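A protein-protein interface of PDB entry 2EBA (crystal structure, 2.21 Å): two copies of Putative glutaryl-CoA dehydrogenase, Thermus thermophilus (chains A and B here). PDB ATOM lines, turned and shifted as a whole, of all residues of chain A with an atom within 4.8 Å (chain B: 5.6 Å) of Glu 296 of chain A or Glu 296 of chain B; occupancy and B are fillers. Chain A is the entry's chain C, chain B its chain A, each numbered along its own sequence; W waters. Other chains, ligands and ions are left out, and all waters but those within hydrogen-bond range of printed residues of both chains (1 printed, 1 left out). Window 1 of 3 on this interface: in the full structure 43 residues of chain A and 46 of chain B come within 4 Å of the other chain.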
ATOM      1  N   ALA A 292     -17.057 -17.096  11.231  1.00  0.00           N
ATOM      2  CA  ALA A 292     -15.739 -16.756  10.679  1.00  0.00           C
ATOM      3  C   ALA A 292     -15.846 -15.902   9.429  1.00  0.00           C
ATOM      4  O   ALA A 292     -15.128 -14.914   9.296  1.00  0.00           O
ATOM      5  CB  ALA A 292     -14.972 -17.992  10.370  1.00  0.00           C
ATOM      6  N   TRP A 293     -16.747 -16.269   8.521  1.00  0.00           N
ATOM      7  CA  TRP A 293     -16.887 -15.512   7.296  1.00  0.00           C
ATOM      8  C   TRP A 293     -17.420 -14.113   7.592  1.00  0.00           C
ATOM      9  O   TRP A 293     -16.932 -13.153   6.982  1.00  0.00           O
ATOM     10  CB  TRP A 293     -17.811 -16.211   6.287  1.00  0.00           C
ATOM     11  CG  TRP A 293     -17.380 -17.587   5.808  1.00  0.00           C
ATOM     12  CD1 TRP A 293     -16.098 -18.053   5.619  1.00  0.00           C
ATOM     13  CD2 TRP A 293     -18.245 -18.636   5.343  1.00  0.00           C
ATOM     14  NE1 TRP A 293     -16.123 -19.318   5.064  1.00  0.00           N
ATOM     15  CE2 TRP A 293     -17.434 -19.701   4.881  1.00  0.00           C
ATOM     16  CE3 TRP A 293     -19.639 -18.778   5.269  1.00  0.00           C
ATOM     17  CZ2 TRP A 293     -17.964 -20.894   4.354  1.00  0.00           C
ATOM     18  CZ3 TRP A 293     -20.169 -19.959   4.748  1.00  0.00           C
ATOM     19  CH2 TRP A 293     -19.332 -20.995   4.299  1.00  0.00           C
ATOM     20  N   HIS A 294     -18.397 -13.979   8.509  1.00  0.00           N
ATOM     21  CA  HIS A 294     -18.946 -12.657   8.840  1.00  0.00           C
ATOM     22  C   HIS A 294     -17.821 -11.695   9.245  1.00  0.00           C
ATOM     23  O   HIS A 294     -17.790 -10.539   8.820  1.00  0.00           O
ATOM     24  CB  HIS A 294     -19.996 -12.744   9.955  1.00  0.00           C
ATOM     25  CG  HIS A 294     -20.795 -11.490  10.146  1.00  0.00           C
ATOM     26  ND1 HIS A 294     -20.443 -10.520  11.053  1.00  0.00           N
ATOM     27  CD2 HIS A 294     -21.904 -11.034   9.520  1.00  0.00           C
ATOM     28  CE1 HIS A 294     -21.294  -9.508  10.966  1.00  0.00           C
ATOM     29  NE2 HIS A 294     -22.189  -9.795  10.039  1.00  0.00           N
ATOM     30  N   THR A 295     -16.905 -12.189  10.075  1.00  0.00           N
ATOM     31  CA  THR A 295     -15.770 -11.402  10.552  1.00  0.00           C
ATOM     32  C   THR A 295     -14.807 -11.019   9.438  1.00  0.00           C
ATOM     33  O   THR A 295     -14.331  -9.891   9.392  1.00  0.00           O
ATOM     34  CB  THR A 295     -15.006 -12.182  11.639  1.00  0.00           C
ATOM     35  OG1 THR A 295     -15.897 -12.468  12.727  1.00  0.00           O
ATOM     36  CG2 THR A 295     -13.830 -11.389  12.146  1.00  0.00           C
ATOM     37  N   GLU A 296     -14.503 -11.965   8.558  1.00  0.00           N
ATOM     38  CA  GLU A 296     -13.602 -11.699   7.436  1.00  0.00           C
ATOM     39  C   GLU A 296     -14.209 -10.634   6.513  1.00  0.00           C
ATOM     40  O   GLU A 296     -13.522  -9.701   6.080  1.00  0.00           O
ATOM     41  CB  GLU A 296     -13.347 -12.995   6.647  1.00  0.00           C
ATOM     42  CG  GLU A 296     -12.499 -14.000   7.407  1.00  0.00           C
ATOM     43  CD  GLU A 296     -12.448 -15.379   6.756  1.00  0.00           C
ATOM     44  OE1 GLU A 296     -11.576 -16.163   7.163  1.00  0.00           O
ATOM     45  OE2 GLU A 296     -13.269 -15.684   5.863  1.00  0.00           O
ATOM     46  N   GLY A 297     -15.504 -10.786   6.242  1.00  0.00           N
ATOM     47  CA  GLY A 297     -16.227  -9.884   5.373  1.00  0.00           C
ATOM     48  C   GLY A 297     -16.266  -8.457   5.853  1.00  0.00           C
ATOM     49  O   GLY A 297     -16.040  -7.547   5.066  1.00  0.00           O
ATOM     50  N   LEU A 298     -16.553  -8.240   7.131  1.00  0.00           N
ATOM     51  CA  LEU A 298     -16.595  -6.873   7.664  1.00  0.00           C
ATOM     52  C   LEU A 298     -15.262  -6.150   7.554  1.00  0.00           C
ATOM     53  O   LEU A 298     -15.214  -4.948   7.305  1.00  0.00           O
ATOM     54  CB  LEU A 298     -17.033  -6.864   9.127  1.00  0.00           C
ATOM     55  CG  LEU A 298     -18.532  -6.952   9.439  1.00  0.00           C
ATOM     56  CD1 LEU A 298     -18.738  -6.660  10.922  1.00  0.00           C
ATOM     57  CD2 LEU A 298     -19.321  -5.945   8.606  1.00  0.00           C
ATOM     58  N   LEU A 299     -14.174  -6.884   7.753  1.00  0.00           N
ATOM     59  CA  LEU A 299     -12.851  -6.292   7.669  1.00  0.00           C
ATOM     60  C   LEU A 299     -12.540  -5.882   6.249  1.00  0.00           C
ATOM     61  O   LEU A 299     -11.983  -4.822   6.021  1.00  0.00           O
ATOM     62  CB  LEU A 299     -11.796  -7.270   8.175  1.00  0.00           C
ATOM     63  CG  LEU A 299     -11.554  -7.289   9.691  1.00  0.00           C
ATOM     64  CD1 LEU A 299     -10.642  -8.417  10.032  1.00  0.00           C
ATOM     65  CD2 LEU A 299     -10.950  -5.971  10.151  1.00  0.00           C
ATOM     66  N   LEU A 300     -12.878  -6.733   5.288  1.00  0.00           N
ATOM     67  CA  LEU A 300     -12.654  -6.385   3.887  1.00  0.00           C
ATOM     68  C   LEU A 300     -13.445  -5.111   3.568  1.00  0.00           C
ATOM     69  O   LEU A 300     -12.897  -4.153   3.014  1.00  0.00           O
ATOM     70  CB  LEU A 300     -13.127  -7.506   2.946  1.00  0.00           C
ATOM     71  CG  LEU A 300     -12.347  -8.824   2.880  1.00  0.00           C
ATOM     72  CD1 LEU A 300     -12.919  -9.681   1.763  1.00  0.00           C
ATOM     73  CD2 LEU A 300     -10.861  -8.554   2.644  1.00  0.00           C
ATOM     74  N   GLN A 324     -15.746 -12.479  -2.532  1.00  0.00           N
ATOM     75  CA  GLN A 324     -15.681 -13.241  -1.274  1.00  0.00           C
ATOM     76  C   GLN A 324     -16.902 -13.138  -0.402  1.00  0.00           C
ATOM     77  O   GLN A 324     -17.397 -14.147   0.093  1.00  0.00           O
ATOM     78  CB  GLN A 324     -14.533 -12.786  -0.400  1.00  0.00           C
ATOM     79  CG  GLN A 324     -13.140 -13.006  -0.928  1.00  0.00           C
ATOM     80  CD  GLN A 324     -12.900 -14.420  -1.310  1.00  0.00           C
ATOM     81  OE1 GLN A 324     -12.950 -14.775  -2.501  1.00  0.00           O
ATOM     82  NE2 GLN A 324     -12.647 -15.271  -0.302  1.00  0.00           N
ATOM     83  N   LYS A 328     -19.629 -16.140   0.380  1.00  0.00           N
ATOM     84  CA  LYS A 328     -19.821 -16.561   1.761  1.00  0.00           C
ATOM     85  C   LYS A 328     -21.227 -16.415   2.236  1.00  0.00           C
ATOM     86  O   LYS A 328     -21.750 -17.309   2.904  1.00  0.00           O
ATOM     87  CB  LYS A 328     -18.940 -15.796   2.684  1.00  0.00           C
ATOM     88  CG  LYS A 328     -17.603 -16.343   2.569  1.00  0.00           C
ATOM     89  CD  LYS A 328     -16.669 -15.224   2.619  1.00  0.00           C
ATOM     90  CE  LYS A 328     -15.354 -15.809   2.337  1.00  0.00           C
ATOM     91  NZ  LYS A 328     -14.422 -15.020   3.143  1.00  0.00           N
ATOM     92  N   LEU B 291      -4.555 -15.160  -2.990  1.00  0.00           N
ATOM     93  CA  LEU B 291      -4.492 -13.750  -2.668  1.00  0.00           C
ATOM     94  C   LEU B 291      -5.635 -13.341  -1.745  1.00  0.00           C
ATOM     95  O   LEU B 291      -5.434 -12.590  -0.796  1.00  0.00           O
ATOM     96  CB  LEU B 291      -4.525 -12.923  -3.955  1.00  0.00           C
ATOM     97  CG  LEU B 291      -4.333 -11.419  -3.786  1.00  0.00           C
ATOM     98  CD1 LEU B 291      -2.919 -11.119  -3.331  1.00  0.00           C
ATOM     99  CD2 LEU B 291      -4.617 -10.728  -5.093  1.00  0.00           C
ATOM    100  N   ALA B 292      -6.833 -13.841  -2.024  1.00  0.00           N
ATOM    101  CA  ALA B 292      -7.997 -13.514  -1.212  1.00  0.00           C
ATOM    102  C   ALA B 292      -7.764 -13.953   0.220  1.00  0.00           C
ATOM    103  O   ALA B 292      -7.958 -13.188   1.157  1.00  0.00           O
ATOM    104  CB  ALA B 292      -9.249 -14.194  -1.774  1.00  0.00           C
ATOM    105  N   TRP B 293      -7.328 -15.193   0.389  1.00  0.00           N
ATOM    106  CA  TRP B 293      -7.086 -15.708   1.726  1.00  0.00           C
ATOM    107  C   TRP B 293      -6.044 -14.895   2.485  1.00  0.00           C
ATOM    108  O   TRP B 293      -6.210 -14.596   3.656  1.00  0.00           O
ATOM    109  CB  TRP B 293      -6.645 -17.158   1.643  1.00  0.00           C
ATOM    110  CG  TRP B 293      -7.739 -18.084   1.263  1.00  0.00           C
ATOM    111  CD1 TRP B 293      -9.070 -17.887   1.436  1.00  0.00           C
ATOM    112  CD2 TRP B 293      -7.592 -19.396   0.717  1.00  0.00           C
ATOM    113  NE1 TRP B 293      -9.770 -18.998   1.033  1.00  0.00           N
ATOM    114  CE2 TRP B 293      -8.884 -19.941   0.585  1.00  0.00           C
ATOM    115  CE3 TRP B 293      -6.491 -20.167   0.329  1.00  0.00           C
ATOM    116  CZ2 TRP B 293      -9.109 -21.228   0.077  1.00  0.00           C
ATOM    117  CZ3 TRP B 293      -6.709 -21.445  -0.175  1.00  0.00           C
ATOM    118  CH2 TRP B 293      -8.011 -21.962  -0.298  1.00  0.00           C
ATOM    119  N   HIS B 294      -4.964 -14.548   1.804  1.00  0.00           N
ATOM    120  CA  HIS B 294      -3.908 -13.778   2.422  1.00  0.00           C
ATOM    121  C   HIS B 294      -4.398 -12.434   2.926  1.00  0.00           C
ATOM    122  O   HIS B 294      -4.036 -12.013   4.011  1.00  0.00           O
ATOM    123  CB  HIS B 294      -2.758 -13.587   1.442  1.00  0.00           C
ATOM    124  CG  HIS B 294      -1.575 -12.893   2.036  1.00  0.00           C
ATOM    125  ND1 HIS B 294      -1.451 -11.519   2.063  1.00  0.00           N
ATOM    126  CD2 HIS B 294      -0.464 -13.384   2.637  1.00  0.00           C
ATOM    127  CE1 HIS B 294      -0.315 -11.198   2.654  1.00  0.00           C
ATOM    128  NE2 HIS B 294       0.302 -12.307   3.012  1.00  0.00           N
ATOM    129  N   THR B 295      -5.227 -11.764   2.133  1.00  0.00           N
ATOM    130  CA  THR B 295      -5.773 -10.464   2.504  1.00  0.00           C
ATOM    131  C   THR B 295      -6.679 -10.605   3.723  1.00  0.00           C
ATOM    132  O   THR B 295      -6.626  -9.791   4.638  1.00  0.00           O
ATOM    133  CB  THR B 295      -6.571  -9.869   1.325  1.00  0.00           C
ATOM    134  OG1 THR B 295      -5.703  -9.747   0.188  1.00  0.00           O
ATOM    135  CG2 THR B 295      -7.137  -8.513   1.681  1.00  0.00           C
ATOM    136  N   GLU B 296      -7.511 -11.641   3.723  1.00  0.00           N
ATOM    137  CA  GLU B 296      -8.421 -11.909   4.824  1.00  0.00           C
ATOM    138  C   GLU B 296      -7.615 -12.208   6.082  1.00  0.00           C
ATOM    139  O   GLU B 296      -7.924 -11.727   7.163  1.00  0.00           O
ATOM    140  CB  GLU B 296      -9.309 -13.105   4.479  1.00  0.00           C
ATOM    141  CG  GLU B 296     -10.353 -12.793   3.427  1.00  0.00           C
ATOM    142  CD  GLU B 296     -11.107 -14.018   2.955  1.00  0.00           C
ATOM    143  OE1 GLU B 296     -12.151 -13.843   2.294  1.00  0.00           O
ATOM    144  OE2 GLU B 296     -10.653 -15.148   3.227  1.00  0.00           O
ATOM    145  N   GLY B 297      -6.563 -12.994   5.922  1.00  0.00           N
ATOM    146  CA  GLY B 297      -5.733 -13.352   7.053  1.00  0.00           C
ATOM    147  C   GLY B 297      -5.012 -12.196   7.703  1.00  0.00           C
ATOM    148  O   GLY B 297      -4.987 -12.110   8.915  1.00  0.00           O
ATOM    149  N   LEU B 298      -4.412 -11.319   6.909  1.00  0.00           N
ATOM    150  CA  LEU B 298      -3.710 -10.164   7.470  1.00  0.00           C
ATOM    151  C   LEU B 298      -4.636  -9.274   8.279  1.00  0.00           C
ATOM    152  O   LEU B 298      -4.256  -8.773   9.342  1.00  0.00           O
ATOM    153  CB  LEU B 298      -3.069  -9.320   6.373  1.00  0.00           C
ATOM    154  CG  LEU B 298      -1.689  -9.722   5.882  1.00  0.00           C
ATOM    155  CD1 LEU B 298      -1.134  -8.575   5.068  1.00  0.00           C
ATOM    156  CD2 LEU B 298      -0.759 -10.005   7.059  1.00  0.00           C
ATOM    157  N   LEU B 299      -5.846  -9.074   7.776  1.00  0.00           N
ATOM    158  CA  LEU B 299      -6.811  -8.251   8.477  1.00  0.00           C
ATOM    159  C   LEU B 299      -7.168  -8.850   9.830  1.00  0.00           C
ATOM    160  O   LEU B 299      -7.234  -8.135  10.822  1.00  0.00           O
ATOM    161  CB  LEU B 299      -8.064  -8.062   7.621  1.00  0.00           C
ATOM    162  CG  LEU B 299      -8.041  -6.900   6.615  1.00  0.00           C
ATOM    163  CD1 LEU B 299      -9.259  -6.997   5.751  1.00  0.00           C
ATOM    164  CD2 LEU B 299      -8.029  -5.554   7.331  1.00  0.00           C
ATOM    165  N   LEU B 300      -7.398 -10.157   9.876  1.00  0.00           N
ATOM    166  CA  LEU B 300      -7.726 -10.813  11.142  1.00  0.00           C
ATOM    167  C   LEU B 300      -6.574 -10.599  12.123  1.00  0.00           C
ATOM    168  O   LEU B 300      -6.784 -10.199  13.267  1.00  0.00           O
ATOM    169  CB  LEU B 300      -7.942 -12.331  10.954  1.00  0.00           C
ATOM    170  CG  LEU B 300      -9.189 -12.849  10.234  1.00  0.00           C
ATOM    171  CD1 LEU B 300      -9.234 -14.370  10.304  1.00  0.00           C
ATOM    172  CD2 LEU B 300     -10.436 -12.267  10.876  1.00  0.00           C
ATOM    173  N   ALA B 301      -5.363 -10.875  11.639  1.00  0.00           N
ATOM    174  CA  ALA B 301      -4.133 -10.772  12.412  1.00  0.00           C
ATOM    175  C   ALA B 301      -3.909  -9.361  12.918  1.00  0.00           C
ATOM    176  O   ALA B 301      -3.557  -9.158  14.079  1.00  0.00           O
ATOM    177  CB  ALA B 301      -2.956 -11.209  11.559  1.00  0.00           C
ATOM    178  N   GLN B 324      -8.646 -20.219  10.991  1.00  0.00           N
ATOM    179  CA  GLN B 324      -8.790 -19.729   9.618  1.00  0.00           C
ATOM    180  C   GLN B 324      -7.477 -19.564   8.854  1.00  0.00           C
ATOM    181  O   GLN B 324      -7.323 -20.080   7.749  1.00  0.00           O
ATOM    182  CB  GLN B 324      -9.529 -18.388   9.589  1.00  0.00           C
ATOM    183  CG  GLN B 324     -10.968 -18.434  10.051  1.00  0.00           C
ATOM    184  CD  GLN B 324     -11.796 -19.464   9.315  1.00  0.00           C
ATOM    185  OE1 GLN B 324     -11.969 -20.580   9.791  1.00  0.00           O
ATOM    186  NE2 GLN B 324     -12.303 -19.097   8.143  1.00  0.00           N
ATOM    187  N   ASN B 325      -6.527 -18.846   9.438  1.00  0.00           N
ATOM    188  CA  ASN B 325      -5.265 -18.602   8.758  1.00  0.00           C
ATOM    189  C   ASN B 325      -4.421 -19.833   8.459  1.00  0.00           C
ATOM    190  O   ASN B 325      -3.865 -19.959   7.372  1.00  0.00           O
ATOM    191  CB  ASN B 325      -4.429 -17.573   9.540  1.00  0.00           C
ATOM    192  CG  ASN B 325      -5.072 -16.194   9.562  1.00  0.00           C
ATOM    193  OD1 ASN B 325      -4.493 -15.231  10.071  1.00  0.00           O
ATOM    194  ND2 ASN B 325      -6.274 -16.094   9.007  1.00  0.00           N
ATOM    195  N   LYS B 328      -6.085 -21.962   5.692  1.00  0.00           N
ATOM    196  CA  LYS B 328      -5.885 -21.303   4.405  1.00  0.00           C
ATOM    197  C   LYS B 328      -4.472 -21.488   3.893  1.00  0.00           C
ATOM    198  O   LYS B 328      -4.274 -21.786   2.725  1.00  0.00           O
ATOM    199  CB  LYS B 328      -6.230 -19.810   4.514  1.00  0.00           C
ATOM    200  CG  LYS B 328      -7.716 -19.572   4.694  1.00  0.00           C
ATOM    201  CD  LYS B 328      -8.069 -18.128   4.971  1.00  0.00           C
ATOM    202  CE  LYS B 328      -9.554 -18.012   5.200  1.00  0.00           C
ATOM    203  NZ  LYS B 328      -9.911 -16.600   5.495  1.00  0.00           N
HETATM  204  O   HOH W   1     -12.753 -18.107   4.772  1.00  0.00           O
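The side-chain carboxylate (OE1) of Glu 296 of chain B sits at hydrogen-bond distance from the side-chain amide nitrogen (NE2) of Gln 324 of chain A, at 3.0 Å.
The side-chain carboxylate (OE1) of Glu 296 of chain B lies within salt-bridge range of the side-chain amino group (NZ) of Lys 328 of chain A, at 2.7 Å.
The side-chain amide nitrogen (NE2) of Gln 324 of chain B sits at hydrogen-bond distance from the side-chain carboxylate (OE1) of Glu 296 of chain A, at 3.2 Å.
The side-chain amino group (NZ) of Lys 328 of chain B is in salt-bridge range of the side-chain carboxylate (OE2) of Glu 296 of chain A, 3.5 Å away.
The side-chain hydroxyl of Thr 295 of chain B is in hydrogen-bond range of the backbone carbonyl oxygen of Leu 291 of chain B.
OE2 of Glu 296 of chain B is in salt-bridge range of NZ of Lys 328 of chain B.
The side-chain carboxylate of Glu 296 of chain A is in salt-bridge range of the side-chain amino group of Lys 328 of chain A, 3.0 Å away.
Among the printed residues, pairs that only touch across the chains: Ala 292 of chain A with Gln 324 of chain B (3.6 Å), Thr 295 of chain A with Leu 300 of chain B (3.7 Å), Glu 296 of chain A with Glu 296 of chain B (3.8 Å), Leu 299 of chain A with Leu 299 of chain B (3.5 Å), Leu 299 of chain A with Leu 300 of chain B (3.7 Å), Leu 300 of chain A with Thr 295 of chain B (3.8 Å), Leu 300 of chain A with Leu 299 of chain B (3.7 Å) and Gln 324 of chain A with Ala 292 of chain B (3.7 Å).
Printed residues of chain B within 4 Å of Glu 296 of chain A: Glu 296 (3.8 Å), Gln 324 (3.2 Å) and Lys 328 (2.4 Å).
Glu 296 of chain B touches just these residues of chain A: Glu 296 (3.8 Å), Gln 324 (3.0 Å) and Lys 328 (2.7 Å).
Printed residues of chain B within 4 Å of Thr 295 of chain A: Leu 300 (3.7 Å).
Of the printed residues of chain A, Ala 292 of chain B touches Gln 324.
Of the printed residues of chain A, Leu 300 of chain B touches Thr 295 (3.7 Å) and Leu 299 (3.7 Å).
His 294 of chain B touches none of the printed residues of chain A.
Trp 293 of chain A touches none of the printed residues of chain B.
The nearest residue of chain A that does not touch Glu 296 of chain B is Leu 300 of chain A (4.3 Å).
Of the 11 printed residues of chain A, 7 touch a printed residue of chain B.
Hydrophobic or aromatic side chains of chain A that line the printed part of chain B: Ala 292, Leu 299 and Leu 300.
Among the printed residues, 12 pairs touch across the chains.
Ala 292 of chain A touches Gln 324 of chain B, and with the chains exchanged Gln 324 of chain A touches Ala 292 of chain B.
Glu 296 of chain B touches its own counterpart, Glu 296 of chain A.
Leu 299 of chain B touches its own counterpart, Leu 299 of chain A.
Leu 299 of chain A touches Leu 300 of chain B, and with the chains exchanged Leu 300 of chain A touches Leu 299 of chain B.
Positions printed for both chains: 292, 293, 294, 295, 296, 297, 298, 299, 300, 324 and 328.
Water W1 bridges OE2 of Glu 296 of chain A and NZ of Lys 328 of chain B.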
